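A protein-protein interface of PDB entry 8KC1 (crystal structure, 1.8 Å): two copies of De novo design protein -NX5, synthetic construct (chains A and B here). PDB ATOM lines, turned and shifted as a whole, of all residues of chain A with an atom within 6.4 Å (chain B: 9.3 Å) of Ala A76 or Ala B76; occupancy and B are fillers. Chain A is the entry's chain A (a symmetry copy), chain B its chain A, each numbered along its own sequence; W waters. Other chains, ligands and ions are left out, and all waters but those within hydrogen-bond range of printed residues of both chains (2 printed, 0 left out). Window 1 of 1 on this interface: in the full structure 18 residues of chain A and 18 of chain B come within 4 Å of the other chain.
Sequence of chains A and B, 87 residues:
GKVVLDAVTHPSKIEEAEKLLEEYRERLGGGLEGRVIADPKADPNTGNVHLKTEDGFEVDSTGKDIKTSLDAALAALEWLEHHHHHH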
ATOM      1  N   VAL A  59       2.645  10.455 -13.807  1.00  0.00           N
ATOM      2  CA  VAL A  59       4.096  10.325 -13.692  1.00  0.00           C
ATOM      3  C   VAL A  59       4.724  10.679 -15.032  1.00  0.00           C
ATOM      4  O   VAL A  59       4.266  10.205 -16.085  1.00  0.00           O
ATOM      5  CB  VAL A  59       4.536   8.894 -13.333  1.00  0.00           C
ATOM      6  CG1 VAL A  59       6.056   8.864 -13.117  1.00  0.00           C
ATOM      7  CG2 VAL A  59       3.785   8.411 -12.136  1.00  0.00           C
ATOM      8  N   SER A  61       8.657  10.498 -16.668  1.00  0.00           N
ATOM      9  CA  SER A  61       9.874   9.804 -16.304  1.00  0.00           C
ATOM     10  C   SER A  61      10.811   9.903 -17.496  1.00  0.00           C
ATOM     11  O   SER A  61      10.425   9.469 -18.589  1.00  0.00           O
ATOM     12  CB  SER A  61       9.508   8.357 -15.986  1.00  0.00           C
ATOM     13  OG  SER A  61      10.620   7.473 -15.957  1.00  0.00           O
ATOM     14  N   ASP A  71       9.563   1.379 -17.106  1.00  0.00           N
ATOM     15  CA  ASP A  71       9.551   0.538 -15.911  1.00  0.00           C
ATOM     16  C   ASP A  71       9.558   1.419 -14.657  1.00  0.00           C
ATOM     17  O   ASP A  71       8.813   1.156 -13.709  1.00  0.00           O
ATOM     18  CB  ASP A  71      10.773  -0.412 -15.895  1.00  0.00           C
ATOM     19  CG  ASP A  71      10.667  -1.590 -16.860  1.00  0.00           C
ATOM     20  OD1 ASP A  71       9.582  -1.900 -17.390  1.00  0.00           O
ATOM     21  OD2 ASP A  71      11.729  -2.224 -17.100  1.00  0.00           O
ATOM     22  N   ALA A  72      10.432   2.454 -14.631  1.00  0.00           N
ATOM     23  CA  ALA A  72      10.474   3.401 -13.517  1.00  0.00           C
ATOM     24  C   ALA A  72       9.133   4.117 -13.345  1.00  0.00           C
ATOM     25  O   ALA A  72       8.650   4.277 -12.208  1.00  0.00           O
ATOM     26  CB  ALA A  72      11.601   4.398 -13.753  1.00  0.00           C
ATOM     27  N   ALA A  73       8.501   4.504 -14.459  1.00  0.00           N
ATOM     28  CA  ALA A  73       7.208   5.191 -14.401  1.00  0.00           C
ATOM     29  C   ALA A  73       6.129   4.299 -13.804  1.00  0.00           C
ATOM     30  O   ALA A  73       5.338   4.770 -12.980  1.00  0.00           O
ATOM     31  CB  ALA A  73       6.792   5.676 -15.796  1.00  0.00           C
ATOM     32  N   LEU A  74       6.084   3.008 -14.199  1.00  0.00           N
ATOM     33  CA  LEU A  74       5.122   2.063 -13.613  1.00  0.00           C
ATOM     34  C   LEU A  74       5.460   1.735 -12.172  1.00  0.00           C
ATOM     35  O   LEU A  74       4.560   1.429 -11.368  1.00  0.00           O
ATOM     36  CB  LEU A  74       5.094   0.778 -14.403  1.00  0.00           C
ATOM     37  CG  LEU A  74       4.590   0.960 -15.826  1.00  0.00           C
ATOM     38  CD1 LEU A  74       4.909  -0.300 -16.552  1.00  0.00           C
ATOM     39  CD2 LEU A  74       3.116   1.084 -15.718  1.00  0.00           C
ATOM     40  N   ALA A  75       6.752   1.739 -11.844  1.00  0.00           N
ATOM     41  CA  ALA A  75       7.192   1.632 -10.453  1.00  0.00           C
ATOM     42  C   ALA A  75       6.605   2.741  -9.602  1.00  0.00           C
ATOM     43  O   ALA A  75       6.028   2.493  -8.527  1.00  0.00           O
ATOM     44  CB  ALA A  75       8.717   1.686 -10.385  1.00  0.00           C
ATOM     45  N   ALA A  76       6.751   3.986 -10.058  1.00  0.00           N
ATOM     46  CA  ALA A  76       6.171   5.102  -9.319  1.00  0.00           C
ATOM     47  C   ALA A  76       4.655   4.998  -9.247  1.00  0.00           C
ATOM     48  O   ALA A  76       4.064   5.328  -8.216  1.00  0.00           O
ATOM     49  CB  ALA A  76       6.568   6.414  -9.970  1.00  0.00           C
ATOM     50  N   LEU A  77       4.001   4.582 -10.339  1.00  0.00           N
ATOM     51  CA  LEU A  77       2.532   4.453 -10.324  1.00  0.00           C
ATOM     52  C   LEU A  77       2.086   3.400  -9.327  1.00  0.00           C
ATOM     53  O   LEU A  77       1.054   3.550  -8.644  1.00  0.00           O
ATOM     54  CB  LEU A  77       2.013   4.095 -11.728  1.00  0.00           C
ATOM     55  CG  LEU A  77       0.504   3.883 -11.919  1.00  0.00           C
ATOM     56  CD1 LEU A  77      -0.266   5.082 -11.480  1.00  0.00           C
ATOM     57  CD2 LEU A  77       0.160   3.575 -13.350  1.00  0.00           C
ATOM     58  N   GLU A  78       2.807   2.288  -9.255  1.00  0.00           N
ATOM     59  CA  GLU A  78       2.469   1.247  -8.254  1.00  0.00           C
ATOM     60  C   GLU A  78       2.580   1.857  -6.854  1.00  0.00           C
ATOM     61  O   GLU A  78       1.746   1.525  -6.004  1.00  0.00           O
ATOM     62  CB  GLU A  78       3.322  -0.010  -8.409  1.00  0.00           C
ATOM     63  CG  GLU A  78       2.591  -1.291  -8.051  1.00  0.00           C
ATOM     64  CD  GLU A  78       1.291  -1.600  -8.782  1.00  0.00           C
ATOM     65  OE1 GLU A  78       0.516  -2.413  -8.260  1.00  0.00           O
ATOM     66  OE2 GLU A  78       1.059  -1.054  -9.880  1.00  0.00           O
ATOM     67  N   TRP A  79       3.571   2.718  -6.643  1.00  0.00           N
ATOM     68  CA  TRP A  79       3.729   3.287  -5.286  1.00  0.00           C
ATOM     69  C   TRP A  79       2.503   4.137  -4.985  1.00  0.00           C
ATOM     70  O   TRP A  79       1.898   3.940  -3.937  1.00  0.00           O
ATOM     71  CB  TRP A  79       5.000   4.126  -5.203  1.00  0.00           C
ATOM     72  CG  TRP A  79       5.401   4.495  -3.809  1.00  0.00           C
ATOM     73  CD1 TRP A  79       4.820   5.424  -2.997  1.00  0.00           C
ATOM     74  CD2 TRP A  79       6.499   3.943  -3.064  1.00  0.00           C
ATOM     75  NE1 TRP A  79       5.472   5.480  -1.796  1.00  0.00           N
ATOM     76  CE2 TRP A  79       6.507   4.584  -1.808  1.00  0.00           C
ATOM     77  CE3 TRP A  79       7.470   2.976  -3.334  1.00  0.00           C
ATOM     78  CZ2 TRP A  79       7.450   4.284  -0.829  1.00  0.00           C
ATOM     79  CZ3 TRP A  79       8.403   2.681  -2.368  1.00  0.00           C
ATOM     80  CH2 TRP A  79       8.391   3.327  -1.132  1.00  0.00           C
ATOM     81  N   LEU A  80       2.146   5.024  -5.897  1.00  0.00           N
ATOM     82  CA  LEU A  80       1.024   5.956  -5.656  1.00  0.00           C
ATOM     83  C   LEU A  80      -0.275   5.178  -5.462  1.00  0.00           C
ATOM     84  O   LEU A  80      -1.058   5.559  -4.613  1.00  0.00           O
ATOM     85  CB  LEU A  80       0.922   6.900  -6.851  1.00  0.00           C
ATOM     86  CG  LEU A  80       2.111   7.824  -7.089  1.00  0.00           C
ATOM     87  CD1 LEU A  80       1.988   8.510  -8.438  1.00  0.00           C
ATOM     88  CD2 LEU A  80       2.223   8.855  -5.980  1.00  0.00           C
ATOM     89  N   GLU A  81      -0.476   4.104  -6.210  1.00  0.00           N
ATOM     90  CA  GLU A  81      -1.769   3.380  -6.148  1.00  0.00           C
ATOM     91  C   GLU A  81      -1.943   2.661  -4.805  1.00  0.00           C
ATOM     92  O   GLU A  81      -3.066   2.218  -4.537  1.00  0.00           O
ATOM     93  CB  GLU A  81      -1.895   2.455  -7.357  1.00  0.00           C
ATOM     94  CG  GLU A  81      -2.278   3.200  -8.618  1.00  0.00           C
ATOM     95  CD  GLU A  81      -2.308   2.368  -9.883  1.00  0.00           C
ATOM     96  OE1 GLU A  81      -1.500   1.432  -9.995  1.00  0.00           O
ATOM     97  OE2 GLU A  81      -3.135   2.670 -10.754  1.00  0.00           O
ATOM     98  N   LEU B  51      11.608  16.085  -9.767  1.00  0.00           N
ATOM     99  CA  LEU B  51      13.006  16.056  -9.405  1.00  0.00           C
ATOM    100  C   LEU B  51      13.864  15.885 -10.637  1.00  0.00           C
ATOM    101  O   LEU B  51      13.432  15.353 -11.654  1.00  0.00           O
ATOM    102  CB  LEU B  51      13.271  14.992  -8.339  1.00  0.00           C
ATOM    103  CG  LEU B  51      12.819  13.555  -8.449  1.00  0.00           C
ATOM    104  CD1 LEU B  51      13.477  12.920  -9.640  1.00  0.00           C
ATOM    105  CD2 LEU B  51      12.978  12.740  -7.167  1.00  0.00           C
ATOM    106  N   THR B  53      18.141  15.257 -11.657  1.00  0.00           N
ATOM    107  CA  THR B  53      19.524  15.107 -11.243  1.00  0.00           C
ATOM    108  C   THR B  53      20.420  15.755 -12.276  1.00  0.00           C
ATOM    109  O   THR B  53      20.009  16.028 -13.409  1.00  0.00           O
ATOM    110  CB  THR B  53      19.924  13.643 -11.101  1.00  0.00           C
ATOM    111  OG1 THR B  53      19.937  13.041 -12.404  1.00  0.00           O
ATOM    112  CG2 THR B  53      18.890  12.909 -10.276  1.00  0.00           C
ATOM    113  N   PHE B  57      18.477  12.482 -15.155  1.00  0.00           N
ATOM    114  CA  PHE B  57      17.220  11.821 -14.802  1.00  0.00           C
ATOM    115  C   PHE B  57      16.217  12.855 -14.311  1.00  0.00           C
ATOM    116  O   PHE B  57      16.559  13.741 -13.516  1.00  0.00           O
ATOM    117  CB  PHE B  57      17.441  10.762 -13.721  1.00  0.00           C
ATOM    118  CG  PHE B  57      18.368   9.643 -14.132  1.00  0.00           C
ATOM    119  CD1 PHE B  57      18.146   8.939 -15.301  1.00  0.00           C
ATOM    120  CD2 PHE B  57      19.453   9.298 -13.347  1.00  0.00           C
ATOM    121  CE1 PHE B  57      18.990   7.905 -15.682  1.00  0.00           C
ATOM    122  CE2 PHE B  57      20.283   8.285 -13.721  1.00  0.00           C
ATOM    123  CZ  PHE B  57      20.053   7.582 -14.897  1.00  0.00           C
ATOM    124  N   GLU B  58      14.969  12.706 -14.749  1.00  0.00           N
ATOM    125  CA  GLU B  58      13.880  13.566 -14.320  1.00  0.00           C
ATOM    126  C   GLU B  58      12.619  12.742 -14.046  1.00  0.00           C
ATOM    127  O   GLU B  58      12.248  11.835 -14.800  1.00  0.00           O
ATOM    128  CB  GLU B  58      13.601  14.591 -15.406  1.00  0.00           C
ATOM    129  CG  GLU B  58      14.392  15.813 -15.291  1.00  0.00           C
ATOM    130  CD  GLU B  58      13.919  16.878 -16.254  1.00  0.00           C
ATOM    131  OE1 GLU B  58      12.896  17.523 -15.938  1.00  0.00           O
ATOM    132  OE2 GLU B  58      14.560  17.087 -17.308  1.00  0.00           O
ATOM    133  N   VAL B  59      11.912  13.098 -12.985  1.00  0.00           N
ATOM    134  CA  VAL B  59      10.632  12.482 -12.639  1.00  0.00           C
ATOM    135  C   VAL B  59       9.672  13.574 -12.193  1.00  0.00           C
ATOM    136  O   VAL B  59      10.039  14.441 -11.384  1.00  0.00           O
ATOM    137  CB  VAL B  59      10.756  11.468 -11.487  1.00  0.00           C
ATOM    138  CG1 VAL B  59       9.401  10.782 -11.261  1.00  0.00           C
ATOM    139  CG2 VAL B  59      11.844  10.488 -11.779  1.00  0.00           C
ATOM    140  N   ASP B  60       8.455  13.517 -12.700  1.00  0.00           N
ATOM    141  CA  ASP B  60       7.361  14.328 -12.203  1.00  0.00           C
ATOM    142  C   ASP B  60       6.302  13.372 -11.667  1.00  0.00           C
ATOM    143  O   ASP B  60       5.973  12.390 -12.299  1.00  0.00           O
ATOM    144  CB  ASP B  60       6.810  15.219 -13.313  1.00  0.00           C
ATOM    145  CG  ASP B  60       5.999  16.433 -12.782  1.00  0.00           C
ATOM    146  OD1 ASP B  60       4.786  16.312 -12.504  1.00  0.00           O
ATOM    147  OD2 ASP B  60       6.580  17.521 -12.647  1.00  0.00           O
ATOM    148  N   SER B  61       5.763  13.649 -10.492  1.00  0.00           N
ATOM    149  CA  SER B  61       4.931  12.672  -9.823  1.00  0.00           C
ATOM    150  C   SER B  61       3.795  13.436  -9.165  1.00  0.00           C
ATOM    151  O   SER B  61       4.075  14.331  -8.356  1.00  0.00           O
ATOM    152  CB  SER B  61       5.797  11.946  -8.797  1.00  0.00           C
ATOM    153  OG  SER B  61       5.057  11.216  -7.829  1.00  0.00           O
ATOM    154  N   THR B  62       2.571  13.099  -9.548  1.00  0.00           N
ATOM    155  CA  THR B  62       1.326  13.692  -9.042  1.00  0.00           C
ATOM    156  C   THR B  62       0.509  12.609  -8.347  1.00  0.00           C
ATOM    157  O   THR B  62       0.076  11.632  -8.986  1.00  0.00           O
ATOM    158  CB  THR B  62       0.490  14.277 -10.168  1.00  0.00           C
ATOM    159  OG1 THR B  62       1.265  15.226 -10.897  1.00  0.00           O
ATOM    160  CG2 THR B  62      -0.708  14.990  -9.611  1.00  0.00           C
ATOM    161  N   GLY B  63       0.230  12.833  -7.055  1.00  0.00           N
ATOM    162  CA  GLY B  63      -0.510  11.894  -6.243  1.00  0.00           C
ATOM    163  C   GLY B  63      -1.551  12.609  -5.425  1.00  0.00           C
ATOM    164  O   GLY B  63      -1.979  13.702  -5.812  1.00  0.00           O
ATOM    165  N   THR B  68       3.357  11.111  -0.393  1.00  0.00           N
ATOM    166  CA  THR B  68       3.292   9.958  -1.317  1.00  0.00           C
ATOM    167  C   THR B  68       3.888  10.286  -2.672  1.00  0.00           C
ATOM    168  O   THR B  68       4.568   9.443  -3.286  1.00  0.00           O
ATOM    169  CB  THR B  68       1.854   9.480  -1.483  1.00  0.00           C
ATOM    170  OG1 THR B  68       1.322   9.210  -0.182  1.00  0.00           O
ATOM    171  CG2 THR B  68       1.833   8.190  -2.279  1.00  0.00           C
ATOM    172  N   SER B  69       3.595  11.480  -3.187  1.00  0.00           N
ATOM    173  CA  SER B  69       4.185  11.914  -4.446  1.00  0.00           C
ATOM    174  C   SER B  69       5.702  11.816  -4.378  1.00  0.00           C
ATOM    175  O   SER B  69       6.345  11.286  -5.278  1.00  0.00           O
ATOM    176  CB  SER B  69       3.795  13.358  -4.731  1.00  0.00           C
ATOM    177  OG  SER B  69       2.499  13.454  -5.269  1.00  0.00           O
ATOM    178  N   LEU B  70       6.283  12.318  -3.298  1.00  0.00           N
ATOM    179  CA  LEU B  70       7.735  12.382  -3.194  1.00  0.00           C
ATOM    180  C   LEU B  70       8.326  10.991  -3.126  1.00  0.00           C
ATOM    181  O   LEU B  70       9.319  10.684  -3.803  1.00  0.00           O
ATOM    182  CB  LEU B  70       8.122  13.199  -1.944  1.00  0.00           C
ATOM    183  CG  LEU B  70       9.607  13.458  -1.637  1.00  0.00           C
ATOM    184  CD1 LEU B  70      10.318  13.976  -2.856  1.00  0.00           C
ATOM    185  CD2 LEU B  70       9.798  14.387  -0.453  1.00  0.00           C
ATOM    186  N   ASP B  71       7.765  10.147  -2.252  1.00  0.00           N
ATOM    187  CA  ASP B  71       8.283   8.791  -2.089  1.00  0.00           C
ATOM    188  C   ASP B  71       8.242   8.055  -3.433  1.00  0.00           C
ATOM    189  O   ASP B  71       9.205   7.373  -3.797  1.00  0.00           O
ATOM    190  CB  ASP B  71       7.459   8.010  -1.035  1.00  0.00           C
ATOM    191  CG  ASP B  71       7.744   8.412   0.410  1.00  0.00           C
ATOM    192  OD1 ASP B  71       8.744   9.095   0.709  1.00  0.00           O
ATOM    193  OD2 ASP B  71       6.916   8.029   1.279  1.00  0.00           O
ATOM    194  N   ALA B  72       7.106   8.159  -4.162  1.00  0.00           N
ATOM    195  CA  ALA B  72       6.984   7.559  -5.491  1.00  0.00           C
ATOM    196  C   ALA B  72       8.030   8.122  -6.454  1.00  0.00           C
ATOM    197  O   ALA B  72       8.651   7.361  -7.219  1.00  0.00           O
ATOM    198  CB  ALA B  72       5.573   7.792  -6.015  1.00  0.00           C
ATOM    199  N   ALA B  73       8.270   9.437  -6.392  1.00  0.00           N
ATOM    200  CA  ALA B  73       9.258  10.073  -7.268  1.00  0.00           C
ATOM    201  C   ALA B  73      10.662   9.554  -6.992  1.00  0.00           C
ATOM    202  O   ALA B  73      11.407   9.284  -7.940  1.00  0.00           O
ATOM    203  CB  ALA B  73       9.210  11.599  -7.116  1.00  0.00           C
ATOM    204  N   LEU B  74      11.040   9.401  -5.705  1.00  0.00           N
ATOM    205  CA  LEU B  74      12.351   8.833  -5.355  1.00  0.00           C
ATOM    206  C   LEU B  74      12.429   7.354  -5.679  1.00  0.00           C
ATOM    207  O   LEU B  74      13.520   6.830  -5.970  1.00  0.00           O
ATOM    208  CB  LEU B  74      12.632   9.017  -3.885  1.00  0.00           C
ATOM    209  CG  LEU B  74      12.758  10.476  -3.477  1.00  0.00           C
ATOM    210  CD1 LEU B  74      12.723  10.504  -1.988  1.00  0.00           C
ATOM    211  CD2 LEU B  74      14.105  10.905  -3.926  1.00  0.00           C
ATOM    212  N   ALA B  75      11.296   6.658  -5.580  1.00  0.00           N
ATOM    213  CA  ALA B  75      11.199   5.277  -6.050  1.00  0.00           C
ATOM    214  C   ALA B  75      11.556   5.169  -7.521  1.00  0.00           C
ATOM    215  O   ALA B  75      12.383   4.330  -7.924  1.00  0.00           O
ATOM    216  CB  ALA B  75       9.783   4.750  -5.826  1.00  0.00           C
ATOM    217  N   ALA B  76      10.930   6.005  -8.350  1.00  0.00           N
ATOM    218  CA  ALA B  76      11.256   5.994  -9.772  1.00  0.00           C
ATOM    219  C   ALA B  76      12.707   6.377 -10.018  1.00  0.00           C
ATOM    220  O   ALA B  76      13.353   5.809 -10.901  1.00  0.00           O
ATOM    221  CB  ALA B  76      10.337   6.943 -10.520  1.00  0.00           C
ATOM    222  N   LEU B  77      13.230   7.364  -9.279  1.00  0.00           N
ATOM    223  CA  LEU B  77      14.635   7.771  -9.466  1.00  0.00           C
ATOM    224  C   LEU B  77      15.584   6.642  -9.114  1.00  0.00           C
ATOM    225  O   LEU B  77      16.627   6.444  -9.766  1.00  0.00           O
ATOM    226  CB  LEU B  77      14.951   9.007  -8.605  1.00  0.00           C
ATOM    227  CG  LEU B  77      16.379   9.573  -8.632  1.00  0.00           C
ATOM    228  CD1 LEU B  77      16.794   9.914 -10.022  1.00  0.00           C
ATOM    229  CD2 LEU B  77      16.512  10.795  -7.765  1.00  0.00           C
ATOM    230  N   GLU B  78      15.287   5.911  -8.046  1.00  0.00           N
ATOM    231  CA  GLU B  78      16.133   4.747  -7.684  1.00  0.00           C
ATOM    232  C   GLU B  78      16.111   3.746  -8.842  1.00  0.00           C
ATOM    233  O   GLU B  78      17.160   3.150  -9.119  1.00  0.00           O
ATOM    234  CB  GLU B  78      15.716   4.112  -6.360  1.00  0.00           C
ATOM    235  CG  GLU B  78      16.875   3.535  -5.569  1.00  0.00           C
ATOM    236  CD  GLU B  78      18.033   4.460  -5.219  1.00  0.00           C
ATOM    237  OE1 GLU B  78      19.115   3.939  -4.917  1.00  0.00           O
ATOM    238  OE2 GLU B  78      17.855   5.695  -5.222  1.00  0.00           O
ATOM    239  N   TRP B  79      14.960   3.584  -9.486  1.00  0.00           N
ATOM    240  CA  TRP B  79      14.900   2.589 -10.579  1.00  0.00           C
ATOM    241  C   TRP B  79      15.822   3.057 -11.695  1.00  0.00           C
ATOM    242  O   TRP B  79      16.654   2.272 -12.136  1.00  0.00           O
ATOM    243  CB  TRP B  79      13.470   2.439 -11.088  1.00  0.00           C
ATOM    244  CG  TRP B  79      13.257   1.255 -11.978  1.00  0.00           C
ATOM    245  CD1 TRP B  79      13.659   1.107 -13.273  1.00  0.00           C
ATOM    246  CD2 TRP B  79      12.566   0.044 -11.634  1.00  0.00           C
ATOM    247  NE1 TRP B  79      13.275  -0.114 -13.754  1.00  0.00           N
ATOM    248  CE2 TRP B  79      12.602  -0.789 -12.770  1.00  0.00           C
ATOM    249  CE3 TRP B  79      11.924  -0.416 -10.481  1.00  0.00           C
ATOM    250  CZ2 TRP B  79      12.019  -2.053 -12.782  1.00  0.00           C
ATOM    251  CZ3 TRP B  79      11.346  -1.664 -10.494  1.00  0.00           C
ATOM    252  CH2 TRP B  79      11.395  -2.470 -11.630  1.00  0.00           C
ATOM    253  N   LEU B  80      15.687   4.307 -12.104  1.00  0.00           N
ATOM    254  CA  LEU B  80      16.475   4.826 -13.242  1.00  0.00           C
ATOM    255  C   LEU B  80      17.966   4.771 -12.920  1.00  0.00           C
ATOM    256  O   LEU B  80      18.738   4.440 -13.801  1.00  0.00           O
ATOM    257  CB  LEU B  80      16.029   6.260 -13.517  1.00  0.00           C
ATOM    258  CG  LEU B  80      14.584   6.447 -13.966  1.00  0.00           C
ATOM    259  CD1 LEU B  80      14.211   7.918 -13.950  1.00  0.00           C
ATOM    260  CD2 LEU B  80      14.369   5.861 -15.350  1.00  0.00           C
ATOM    261  N   GLU B  81      18.349   5.057 -11.685  1.00  0.00           N
ATOM    262  CA  GLU B  81      19.791   5.133 -11.347  1.00  0.00           C
ATOM    263  C   GLU B  81      20.449   3.750 -11.391  1.00  0.00           C
ATOM    264  O   GLU B  81      21.685   3.705 -11.357  1.00  0.00           O
ATOM    265  CB  GLU B  81      19.964   5.851 -10.010  1.00  0.00           C
ATOM    266  CG  GLU B  81      19.829   7.353 -10.139  1.00  0.00           C
ATOM    267  CD  GLU B  81      19.873   8.125  -8.837  1.00  0.00           C
ATOM    268  OE1 GLU B  81      19.403   7.594  -7.817  1.00  0.00           O
ATOM    269  OE2 GLU B  81      20.370   9.261  -8.853  1.00  0.00           O
ATOM    270  N   HIS B  82      19.666   2.670 -11.463  1.00  0.00           N
ATOM    271  CA  HIS B  82      20.208   1.316 -11.434  1.00  0.00           C
ATOM    272  C   HIS B  82      20.015   0.550 -12.726  1.00  0.00           C
ATOM    273  O   HIS B  82      20.959  -0.107 -13.190  1.00  0.00           O
ATOM    274  CB  HIS B  82      19.601   0.552 -10.264  1.00  0.00           C
ATOM    275  CG  HIS B  82      19.867   1.211  -8.946  1.00  0.00           C
ATOM    276  ND1 HIS B  82      20.624   2.361  -8.841  1.00  0.00           N
ATOM    277  CD2 HIS B  82      19.456   0.915  -7.690  1.00  0.00           C
ATOM    278  CE1 HIS B  82      20.707   2.722  -7.575  1.00  0.00           C
ATOM    279  NE2 HIS B  82      19.993   1.870  -6.856  1.00  0.00           N
ATOM    280  N   HIS B  83      18.841   0.646 -13.345  1.00  0.00           N
ATOM    281  CA  HIS B  83      18.569  -0.183 -14.509  1.00  0.00           C
ATOM    282  C   HIS B  83      19.042   0.412 -15.823  1.00  0.00           C
ATOM    283  O   HIS B  83      19.516  -0.337 -16.685  1.00  0.00           O
ATOM    284  CB  HIS B  83      17.079  -0.501 -14.609  1.00  0.00           C
ATOM    285  CG  HIS B  83      16.517  -1.213 -13.414  1.00  0.00           C
ATOM    286  ND1 HIS B  83      16.562  -0.686 -12.140  1.00  0.00           N
ATOM    287  CD2 HIS B  83      15.916  -2.429 -13.303  1.00  0.00           C
ATOM    288  CE1 HIS B  83      15.987  -1.530 -11.300  1.00  0.00           C
ATOM    289  NE2 HIS B  83      15.593  -2.597 -11.978  1.00  0.00           N
HETATM  290  O   HOH W   1      13.968  -1.642 -16.173  1.00  0.00           O
HETATM  291  O   HOH W   2       4.840   6.740   0.788  1.00  0.00           O
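O of Ser B69 lies within hydrogen-bond range of OG of Ser B61 (2.9 Å). O of Trp B79 is in hydrogen-bond range of ND1 of His B83 (3.0 Å). The backbone NH of Gly B63 is in hydrogen-bond range of the side-chain hydroxyl of Ser B69 (3.0 Å).
Among the printed residues, pairs that only touch across the chains: Val A59 with Asp B60 (3.1 Å), Trp A79 with Asp B71 (3.3 Å), Asp A71 with Trp B79 (3.3 Å), Ser A61 with Glu B58 (3.5 Å), Ala A72 with Leu B80 (3.5 Å), Leu A80 with Ala B72 (3.5 Å), Ala A72 with Ala B76 (3.6 Å), Ala A76 with Ala B72 (3.6 Å), Leu A80 with Thr B68 (3.6 Å), Leu A80 with Thr B62 (3.7 Å), Trp A79 with Ala B72 (3.8 Å), Ala A72 with Trp B79 (3.8 Å), Trp A79 with Ala B75 (3.8 Å), Ala A75 with Trp B79 (3.8 Å), Ala A76 with Ala B76 (3.8 Å) and Leu A80 with Ser B69 (3.9 Å).
Printed residues of chain B within 4 Å of Asp A71: Trp B79. Ala A76 touches two residues of chain B. Of the printed residues of chain A, Glu B58 touches Ser A61. Gly B63 touches none of the printed residues of chain A. Of the printed residues of chain A, Asp B71 touches Trp A79. Ala B73 touches none of the printed residues of chain A. Of chain A, only Ala A72 and Ala A76 come within 4 Å of Ala B76. The nearest residue of chain B that does not touch Ala A76 is Ala B73 (5.0 Å). The nearest printed residue of chain A that does not touch Asp B71 is Leu A80 (6.6 Å).
Of the 13 printed residues of chain A, 8 touch a printed residue of chain B. Hydrophobic or aromatic side chains of chain A that line the printed part of chain B: Val A59, Ala A72, Ala A75, Ala A76, Trp A79 and Leu A80. Of the 25 printed residues of chain B, 11 touch a printed residue of chain A. Hydrophobic or aromatic side chains of chain B that line the printed part of chain A: Ala B72, Ala B75, Ala B76, Trp B79 and Leu B80.
Asp A71 touches Trp B79, and with the chains exchanged Trp A79 touches Asp B71. Ala A72 touches Leu B80, and with the chains exchanged Leu A80 touches Ala B72. Ala A75 touches Trp B79, and with the chains exchanged Trp A79 touches Ala B75. Ala B76 touches its own counterpart, Ala A76.
Water W1 lies within hydrogen-bond range of the side-chain carboxylate (OD2) of Asp A71 (2.5 Å) and the indole nitrogen (NE1) of Trp B79 (2.9 Å). Water W2 bridges the side-chain carboxylate of Asp B71 (2.5 Å) and the indole nitrogen of Trp A79 (2.9 Å).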
